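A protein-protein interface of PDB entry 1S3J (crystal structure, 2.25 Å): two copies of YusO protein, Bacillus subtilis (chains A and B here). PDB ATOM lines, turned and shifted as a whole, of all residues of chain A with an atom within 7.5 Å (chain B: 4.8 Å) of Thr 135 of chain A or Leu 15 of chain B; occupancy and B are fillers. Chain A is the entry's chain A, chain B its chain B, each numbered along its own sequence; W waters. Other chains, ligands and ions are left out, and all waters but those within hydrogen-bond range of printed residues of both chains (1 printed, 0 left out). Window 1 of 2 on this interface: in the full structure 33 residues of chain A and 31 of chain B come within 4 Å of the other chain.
The backbone carbonyl oxygen (O) of Ala 131 of chain A lies within hydrogen-bond range of the side-chain hydroxyl (OG1) of Thr 135 of chain A (2.6 Å).
OG1 of Thr 135 of chain A lies within hydrogen-bond range of O of Ala 132 of chain A, at 3.2 Å.
Printed residues of chain B that touch a printed residue of chain A: Ile 11, Gln 12, Ser 14, Leu 15, Gln 16 and Leu 18.
Hydrophobic or aromatic side chains of chain B within 4 Å of the printed part of chain A: Ile 11, Leu 15 and Leu 18.
Along chain B the printed residues that touch a printed residue of chain A span positions 11 to 18.
Of the 19 printed residues of chain A, 9 touch a printed residue of chain B.
Among the printed residues, no Asp or Glu carboxylate lies within 4 Å of a Lys or Arg side-chain nitrogen of the other chain.
NH1 of Arg 112 of chain A touches OE1 of Gln 12 of chain B, 3.7 Å away.
Met 116 of chain A touches Gln 12 of chain B (CB to NE2, 3.5 Å).
CD1 of Leu 120 of chain A touches CG2 of Ile 11 of chain B, at 3.6 Å.
Met 128 of chain A touches Ile 11 of chain B.
CG1 of Ile 11 of chain B touches CA of Ala 132 of chain A, 3.7 Å away.
O of Thr 135 of chain A touches CB of Ser 14 of chain B, at 3.5 Å.
Thr 135 of chain A touches Leu 15 of chain B (CG2 to CD2, 3.7 Å).
Thr 135 of chain A touches Leu 18 of chain B.
Leu 138 of chain A touches Leu 18 of chain B (O to CD2, 3.6 Å).
CB of Ala 139 of chain A touches O of Ser 14 of chain B (3.97 Å).
Position printed for both chains: 15.
Of the 14 pairs that touch across the chains among the printed residues, none has its exchanged pair printed and touching as well.
Printed residues of chain B within 4 Å of Thr 135 of chain A: Ser 14, Leu 15 and Leu 18.
Of the printed residues of chain A, Leu 15 of chain B touches Met 116 (3.8 Å) and Thr 135 (3.7 Å).
Printed residues of chain B within 4 Å of Ala 139 of chain A: Ser 14 (3.97 Å) and Leu 18 (3.8 Å).
Of the printed residues of chain A, Ile 11 of chain B touches Leu 120, Met 128 and Ala 132.
Ala 141 of chain A touches none of the printed residues of chain B.
The nearest printed residue of chain B that does not touch Thr 135 of chain A is Ile 11 of chain B (4.02 Å).
The nearest residue of chain A that does not touch Leu 15 of chain B is Leu 120 of chain A (5.5 Å).
The nearest printed residue of chain B that does not touch Met 116 of chain A is Ile 11 of chain B (4.9 Å).
Water W1 lies within hydrogen-bond range of OG of Ser 14 of chain B (2.7 Å), O of Ala 132 of chain A (3.0 Å) and OG1 of Thr 135 of chain A (3.0 Å).
NH1 of Arg 112 of chain A lies within hydrogen-bond range of OE1 of Gln 16 of chain B, 2.7 Å away.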
ATOM      1  N   LEU A  15       1.756 -16.108 -31.101  1.00  0.00           N
ATOM      2  CA  LEU A  15       1.941 -17.113 -30.057  1.00  0.00           C
ATOM      3  C   LEU A  15       0.664 -17.887 -29.773  1.00  0.00           C
ATOM      4  O   LEU A  15       0.709 -19.092 -29.599  1.00  0.00           O
ATOM      5  CB  LEU A  15       2.514 -16.496 -28.777  1.00  0.00           C
ATOM      6  CG  LEU A  15       3.934 -15.942 -28.921  1.00  0.00           C
ATOM      7  CD1 LEU A  15       4.355 -15.259 -27.662  1.00  0.00           C
ATOM      8  CD2 LEU A  15       4.900 -17.021 -29.266  1.00  0.00           C
ATOM      9  N   ILE A  22      -0.091 -26.326 -31.347  1.00  0.00           N
ATOM     10  CA  ILE A  22       1.005 -27.185 -30.903  1.00  0.00           C
ATOM     11  C   ILE A  22       0.649 -27.894 -29.609  1.00  0.00           C
ATOM     12  O   ILE A  22       1.029 -29.045 -29.422  1.00  0.00           O
ATOM     13  CB  ILE A  22       2.325 -26.388 -30.748  1.00  0.00           C
ATOM     14  CG1 ILE A  22       2.920 -26.061 -32.116  1.00  0.00           C
ATOM     15  CG2 ILE A  22       3.381 -27.177 -29.964  1.00  0.00           C
ATOM     16  CD1 ILE A  22       3.894 -24.878 -32.098  1.00  0.00           C
ATOM     17  N   ARG A 112       8.129 -34.850 -28.745  1.00  0.00           N
ATOM     18  CA  ARG A 112       7.978 -33.393 -28.630  1.00  0.00           C
ATOM     19  C   ARG A 112       8.903 -32.643 -29.591  1.00  0.00           C
ATOM     20  O   ARG A 112       8.530 -31.604 -30.133  1.00  0.00           O
ATOM     21  CB  ARG A 112       8.277 -32.893 -27.210  1.00  0.00           C
ATOM     22  CG  ARG A 112       7.222 -33.215 -26.171  1.00  0.00           C
ATOM     23  CD  ARG A 112       7.615 -32.757 -24.760  1.00  0.00           C
ATOM     24  NE  ARG A 112       6.460 -32.371 -23.946  1.00  0.00           N
ATOM     25  CZ  ARG A 112       6.037 -31.133 -23.744  1.00  0.00           C
ATOM     26  NH1 ARG A 112       6.653 -30.097 -24.293  1.00  0.00           N
ATOM     27  NH2 ARG A 112       4.976 -30.921 -22.987  1.00  0.00           N
ATOM     28  N   MET A 116       7.935 -30.007 -32.772  1.00  0.00           N
ATOM     29  CA  MET A 116       8.469 -28.643 -32.822  1.00  0.00           C
ATOM     30  C   MET A 116       9.242 -28.410 -34.104  1.00  0.00           C
ATOM     31  O   MET A 116       9.102 -27.376 -34.734  1.00  0.00           O
ATOM     32  CB  MET A 116       9.388 -28.371 -31.619  1.00  0.00           C
ATOM     33  CG  MET A 116       9.846 -26.912 -31.504  1.00  0.00           C
ATOM     34  SD  MET A 116       8.361 -25.639 -31.371  1.00  0.00           S
ATOM     35  CE  MET A 116       7.156 -26.643 -30.303  1.00  0.00           C
ATOM     36  N   LEU A 120       9.755 -25.486 -36.879  1.00  0.00           N
ATOM     37  CA  LEU A 120      11.030 -24.776 -36.933  1.00  0.00           C
ATOM     38  C   LEU A 120      11.735 -24.913 -38.272  1.00  0.00           C
ATOM     39  O   LEU A 120      12.517 -24.043 -38.648  1.00  0.00           O
ATOM     40  CB  LEU A 120      11.958 -25.260 -35.813  1.00  0.00           C
ATOM     41  CG  LEU A 120      11.457 -24.939 -34.405  1.00  0.00           C
ATOM     42  CD1 LEU A 120      12.414 -25.485 -33.341  1.00  0.00           C
ATOM     43  CD2 LEU A 120      11.222 -23.436 -34.223  1.00  0.00           C
ATOM     44  N   MET A 128      16.818 -19.438 -37.524  1.00  0.00           N
ATOM     45  CA  MET A 128      17.049 -20.520 -36.551  1.00  0.00           C
ATOM     46  C   MET A 128      18.050 -20.093 -35.476  1.00  0.00           C
ATOM     47  O   MET A 128      17.843 -20.367 -34.302  1.00  0.00           O
ATOM     48  CB  MET A 128      17.541 -21.787 -37.250  1.00  0.00           C
ATOM     49  CG  MET A 128      17.526 -23.032 -36.382  1.00  0.00           C
ATOM     50  SD  MET A 128      15.697 -23.739 -36.247  1.00  0.00           S
ATOM     51  CE  MET A 128      15.491 -24.434 -38.070  1.00  0.00           C
ATOM     52  N   LEU A 129      19.139 -19.448 -35.890  1.00  0.00           N
ATOM     53  CA  LEU A 129      20.180 -19.013 -34.970  1.00  0.00           C
ATOM     54  C   LEU A 129      19.622 -17.912 -34.055  1.00  0.00           C
ATOM     55  O   LEU A 129      19.848 -17.950 -32.850  1.00  0.00           O
ATOM     56  CB  LEU A 129      21.403 -18.485 -35.706  1.00  0.00           C
ATOM     57  CG  LEU A 129      22.288 -19.551 -36.341  1.00  0.00           C
ATOM     58  CD1 LEU A 129      23.014 -18.963 -37.533  1.00  0.00           C
ATOM     59  CD2 LEU A 129      23.281 -20.122 -35.314  1.00  0.00           C
ATOM     60  N   GLN A 130      18.883 -16.966 -34.642  1.00  0.00           N
ATOM     61  CA  GLN A 130      18.186 -15.931 -33.873  1.00  0.00           C
ATOM     62  C   GLN A 130      17.259 -16.581 -32.859  1.00  0.00           C
ATOM     63  O   GLN A 130      17.252 -16.171 -31.708  1.00  0.00           O
ATOM     64  CB  GLN A 130      17.346 -15.038 -34.774  1.00  0.00           C
ATOM     65  CG  GLN A 130      18.111 -14.074 -35.669  1.00  0.00           C
ATOM     66  CD  GLN A 130      17.244 -13.486 -36.770  1.00  0.00           C
ATOM     67  OE1 GLN A 130      16.032 -13.661 -36.770  1.00  0.00           O
ATOM     68  NE2 GLN A 130      17.858 -12.774 -37.686  1.00  0.00           N
ATOM     69  N   ALA A 131      16.484 -17.603 -33.270  1.00  0.00           N
ATOM     70  CA  ALA A 131      15.512 -18.220 -32.351  1.00  0.00           C
ATOM     71  C   ALA A 131      16.208 -18.969 -31.223  1.00  0.00           C
ATOM     72  O   ALA A 131      15.730 -18.970 -30.110  1.00  0.00           O
ATOM     73  CB  ALA A 131      14.519 -19.160 -33.087  1.00  0.00           C
ATOM     74  N   ALA A 132      17.327 -19.613 -31.514  1.00  0.00           N
ATOM     75  CA  ALA A 132      18.119 -20.286 -30.472  1.00  0.00           C
ATOM     76  C   ALA A 132      18.521 -19.292 -29.407  1.00  0.00           C
ATOM     77  O   ALA A 132      18.334 -19.547 -28.228  1.00  0.00           O
ATOM     78  CB  ALA A 132      19.360 -20.932 -31.045  1.00  0.00           C
ATOM     79  N   HIS A 133      19.070 -18.165 -29.854  1.00  0.00           N
ATOM     80  CA  HIS A 133      19.587 -17.122 -28.972  1.00  0.00           C
ATOM     81  C   HIS A 133      18.484 -16.424 -28.136  1.00  0.00           C
ATOM     82  O   HIS A 133      18.650 -16.213 -26.961  1.00  0.00           O
ATOM     83  CB  HIS A 133      20.304 -16.068 -29.816  1.00  0.00           C
ATOM     84  CG  HIS A 133      20.783 -14.892 -29.034  1.00  0.00           C
ATOM     85  ND1 HIS A 133      20.037 -13.739 -28.882  1.00  0.00           N
ATOM     86  CD2 HIS A 133      21.936 -14.691 -28.351  1.00  0.00           C
ATOM     87  CE1 HIS A 133      20.715 -12.882 -28.141  1.00  0.00           C
ATOM     88  NE2 HIS A 133      21.867 -13.434 -27.805  1.00  0.00           N
ATOM     89  N   ILE A 134      17.388 -16.031 -28.774  1.00  0.00           N
ATOM     90  CA  ILE A 134      16.265 -15.376 -28.096  1.00  0.00           C
ATOM     91  C   ILE A 134      15.585 -16.317 -27.074  1.00  0.00           C
ATOM     92  O   ILE A 134      15.284 -15.904 -25.973  1.00  0.00           O
ATOM     93  CB  ILE A 134      15.276 -14.869 -29.156  1.00  0.00           C
ATOM     94  CG1 ILE A 134      15.915 -13.736 -29.977  1.00  0.00           C
ATOM     95  CG2 ILE A 134      13.980 -14.422 -28.563  1.00  0.00           C
ATOM     96  CD1 ILE A 134      15.135 -13.407 -31.251  1.00  0.00           C
ATOM     97  N   THR A 135      15.336 -17.572 -27.425  1.00  0.00           N
ATOM     98  CA  THR A 135      14.670 -18.464 -26.487  1.00  0.00           C
ATOM     99  C   THR A 135      15.573 -18.812 -25.293  1.00  0.00           C
ATOM    100  O   THR A 135      15.082 -18.867 -24.158  1.00  0.00           O
ATOM    101  CB  THR A 135      14.201 -19.748 -27.133  1.00  0.00           C
ATOM    102  OG1 THR A 135      15.265 -20.317 -27.896  1.00  0.00           O
ATOM    103  CG2 THR A 135      13.047 -19.496 -28.114  1.00  0.00           C
ATOM    104  N   ALA A 136      16.866 -19.022 -25.554  1.00  0.00           N
ATOM    105  CA  ALA A 136      17.847 -19.273 -24.502  1.00  0.00           C
ATOM    106  C   ALA A 136      17.961 -18.065 -23.568  1.00  0.00           C
ATOM    107  O   ALA A 136      17.929 -18.216 -22.351  1.00  0.00           O
ATOM    108  CB  ALA A 136      19.224 -19.629 -25.095  1.00  0.00           C
ATOM    109  N   LYS A 137      18.042 -16.876 -24.132  1.00  0.00           N
ATOM    110  CA  LYS A 137      18.095 -15.666 -23.336  1.00  0.00           C
ATOM    111  C   LYS A 137      16.810 -15.436 -22.511  1.00  0.00           C
ATOM    112  O   LYS A 137      16.873 -15.056 -21.330  1.00  0.00           O
ATOM    113  CB  LYS A 137      18.347 -14.469 -24.247  1.00  0.00           C
ATOM    114  CG  LYS A 137      18.351 -13.151 -23.536  1.00  0.00           C
ATOM    115  CD  LYS A 137      18.866 -12.045 -24.450  1.00  0.00           C
ATOM    116  CE  LYS A 137      18.918 -10.688 -23.725  1.00  0.00           C
ATOM    117  NZ  LYS A 137      19.111  -9.560 -24.699  1.00  0.00           N
ATOM    118  N   LEU A 138      15.648 -15.664 -23.116  1.00  0.00           N
ATOM    119  CA  LEU A 138      14.396 -15.537 -22.373  1.00  0.00           C
ATOM    120  C   LEU A 138      14.323 -16.573 -21.253  1.00  0.00           C
ATOM    121  O   LEU A 138      13.857 -16.275 -20.166  1.00  0.00           O
ATOM    122  CB  LEU A 138      13.187 -15.719 -23.301  1.00  0.00           C
ATOM    123  CG  LEU A 138      12.909 -14.661 -24.353  1.00  0.00           C
ATOM    124  CD1 LEU A 138      11.781 -15.130 -25.308  1.00  0.00           C
ATOM    125  CD2 LEU A 138      12.521 -13.406 -23.674  1.00  0.00           C
ATOM    126  N   ALA A 139      14.764 -17.796 -21.535  1.00  0.00           N
ATOM    127  CA  ALA A 139      14.664 -18.885 -20.571  1.00  0.00           C
ATOM    128  C   ALA A 139      15.621 -18.651 -19.376  1.00  0.00           C
ATOM    129  O   ALA A 139      15.258 -18.935 -18.227  1.00  0.00           O
ATOM    130  CB  ALA A 139      14.955 -20.191 -21.225  1.00  0.00           C
ATOM    131  N   GLN A 140      16.817 -18.134 -19.658  1.00  0.00           N
ATOM    132  CA  GLN A 140      17.794 -17.745 -18.636  1.00  0.00           C
ATOM    133  C   GLN A 140      17.237 -16.627 -17.739  1.00  0.00           C
ATOM    134  O   GLN A 140      17.267 -16.745 -16.531  1.00  0.00           O
ATOM    135  CB  GLN A 140      19.109 -17.265 -19.283  1.00  0.00           C
ATOM    136  CG  GLN A 140      20.281 -17.053 -18.307  1.00  0.00           C
ATOM    137  CD  GLN A 140      21.581 -16.588 -18.988  1.00  0.00           C
ATOM    138  OE1 GLN A 140      22.040 -17.184 -19.981  1.00  0.00           O
ATOM    139  NE2 GLN A 140      22.182 -15.522 -18.446  1.00  0.00           N
ATOM    140  N   ALA A 141      16.748 -15.551 -18.339  1.00  0.00           N
ATOM    141  CA  ALA A 141      16.230 -14.424 -17.570  1.00  0.00           C
ATOM    142  C   ALA A 141      15.034 -14.827 -16.695  1.00  0.00           C
ATOM    143  O   ALA A 141      14.893 -14.320 -15.587  1.00  0.00           O
ATOM    144  CB  ALA A 141      15.838 -13.306 -18.474  1.00  0.00           C
ATOM    145  N   ILE B  11      16.238 -25.142 -28.760  1.00  0.00           N
ATOM    146  CA  ILE B  11      15.072 -24.278 -28.845  1.00  0.00           C
ATOM    147  C   ILE B  11      13.916 -24.923 -28.107  1.00  0.00           C
ATOM    148  O   ILE B  11      13.255 -24.271 -27.306  1.00  0.00           O
ATOM    149  CB  ILE B  11      14.708 -24.007 -30.311  1.00  0.00           C
ATOM    150  CG1 ILE B  11      15.655 -22.954 -30.902  1.00  0.00           C
ATOM    151  CG2 ILE B  11      13.249 -23.551 -30.431  1.00  0.00           C
ATOM    152  CD1 ILE B  11      15.794 -23.010 -32.380  1.00  0.00           C
ATOM    153  N   GLN B  12      13.709 -26.215 -28.344  1.00  0.00           N
ATOM    154  CA  GLN B  12      12.628 -26.975 -27.701  1.00  0.00           C
ATOM    155  C   GLN B  12      12.762 -26.929 -26.198  1.00  0.00           C
ATOM    156  O   GLN B  12      11.791 -26.708 -25.490  1.00  0.00           O
ATOM    157  CB  GLN B  12      12.612 -28.431 -28.217  1.00  0.00           C
ATOM    158  CG  GLN B  12      11.743 -29.435 -27.455  1.00  0.00           C
ATOM    159  CD  GLN B  12      10.307 -28.981 -27.264  1.00  0.00           C
ATOM    160  OE1 GLN B  12       9.640 -29.401 -26.300  1.00  0.00           O
ATOM    161  NE2 GLN B  12       9.819 -28.128 -28.172  1.00  0.00           N
ATOM    162  N   LEU B  13      13.976 -27.094 -25.700  1.00  0.00           N
ATOM    163  CA  LEU B  13      14.192 -27.148 -24.271  1.00  0.00           C
ATOM    164  C   LEU B  13      14.047 -25.760 -23.622  1.00  0.00           C
ATOM    165  O   LEU B  13      13.574 -25.647 -22.481  1.00  0.00           O
ATOM    166  CB  LEU B  13      15.550 -27.785 -23.978  1.00  0.00           C
ATOM    167  CG  LEU B  13      15.651 -29.230 -24.508  1.00  0.00           C
ATOM    168  CD1 LEU B  13      17.103 -29.747 -24.513  1.00  0.00           C
ATOM    169  CD2 LEU B  13      14.728 -30.157 -23.699  1.00  0.00           C
ATOM    170  N   SER B  14      14.435 -24.712 -24.350  1.00  0.00           N
ATOM    171  CA  SER B  14      14.184 -23.349 -23.883  1.00  0.00           C
ATOM    172  C   SER B  14      12.672 -23.046 -23.868  1.00  0.00           C
ATOM    173  O   SER B  14      12.166 -22.466 -22.908  1.00  0.00           O
ATOM    174  CB  SER B  14      14.942 -22.330 -24.731  1.00  0.00           C
ATOM    175  OG  SER B  14      16.319 -22.652 -24.802  1.00  0.00           O
ATOM    176  N   LEU B  15      11.951 -23.466 -24.910  1.00  0.00           N
ATOM    177  CA  LEU B  15      10.503 -23.232 -24.986  1.00  0.00           C
ATOM    178  C   LEU B  15       9.783 -23.984 -23.890  1.00  0.00           C
ATOM    179  O   LEU B  15       8.854 -23.447 -23.279  1.00  0.00           O
ATOM    180  CB  LEU B  15       9.928 -23.626 -26.351  1.00  0.00           C
ATOM    181  CG  LEU B  15      10.399 -22.736 -27.500  1.00  0.00           C
ATOM    182  CD1 LEU B  15       9.947 -23.278 -28.851  1.00  0.00           C
ATOM    183  CD2 LEU B  15       9.910 -21.321 -27.327  1.00  0.00           C
ATOM    184  N   GLN B  16      10.231 -25.207 -23.619  1.00  0.00           N
ATOM    185  CA  GLN B  16       9.646 -26.021 -22.565  1.00  0.00           C
ATOM    186  C   GLN B  16       9.844 -25.372 -21.206  1.00  0.00           C
ATOM    187  O   GLN B  16       8.903 -25.328 -20.408  1.00  0.00           O
ATOM    188  CB  GLN B  16      10.211 -27.445 -22.562  1.00  0.00           C
ATOM    189  CG  GLN B  16       9.913 -28.263 -21.270  1.00  0.00           C
ATOM    190  CD  GLN B  16       8.458 -28.677 -21.142  1.00  0.00           C
ATOM    191  OE1 GLN B  16       7.829 -29.026 -22.129  1.00  0.00           O
ATOM    192  NE2 GLN B  16       7.928 -28.651 -19.918  1.00  0.00           N
ATOM    193  N   ALA B  17      11.038 -24.858 -20.933  1.00  0.00           N
ATOM    194  CA  ALA B  17      11.276 -24.198 -19.642  1.00  0.00           C
ATOM    195  C   ALA B  17      10.492 -22.885 -19.543  1.00  0.00           C
ATOM    196  O   ALA B  17      10.066 -22.514 -18.465  1.00  0.00           O
ATOM    197  CB  ALA B  17      12.757 -23.950 -19.430  1.00  0.00           C
ATOM    198  N   LEU B  18      10.299 -22.193 -20.670  1.00  0.00           N
ATOM    199  CA  LEU B  18       9.575 -20.940 -20.673  1.00  0.00           C
ATOM    200  C   LEU B  18       8.085 -21.212 -20.403  1.00  0.00           C
ATOM    201  O   LEU B  18       7.515 -20.651 -19.488  1.00  0.00           O
ATOM    202  CB  LEU B  18       9.764 -20.183 -21.984  1.00  0.00           C
ATOM    203  CG  LEU B  18      11.055 -19.346 -22.142  1.00  0.00           C
ATOM    204  CD1 LEU B  18      11.243 -18.931 -23.581  1.00  0.00           C
ATOM    205  CD2 LEU B  18      11.021 -18.126 -21.276  1.00  0.00           C
ATOM    206  N   PHE B  19       7.492 -22.091 -21.198  1.00  0.00           N
ATOM    207  CA  PHE B  19       6.101 -22.507 -21.064  1.00  0.00           C
ATOM    208  C   PHE B  19       5.715 -23.015 -19.671  1.00  0.00           C
ATOM    209  O   PHE B  19       4.591 -22.780 -19.222  1.00  0.00           O
ATOM    210  CB  PHE B  19       5.792 -23.595 -22.100  1.00  0.00           C
ATOM    211  CG  PHE B  19       4.540 -24.378 -21.811  1.00  0.00           C
ATOM    212  CD1 PHE B  19       3.286 -23.808 -22.017  1.00  0.00           C
ATOM    213  CD2 PHE B  19       4.610 -25.688 -21.351  1.00  0.00           C
ATOM    214  CE1 PHE B  19       2.127 -24.532 -21.749  1.00  0.00           C
ATOM    215  CE2 PHE B  19       3.457 -26.417 -21.089  1.00  0.00           C
ATOM    216  CZ  PHE B  19       2.215 -25.835 -21.286  1.00  0.00           C
HETATM  217  O   HOH W   1      17.511 -22.241 -27.207  1.00  0.00           O
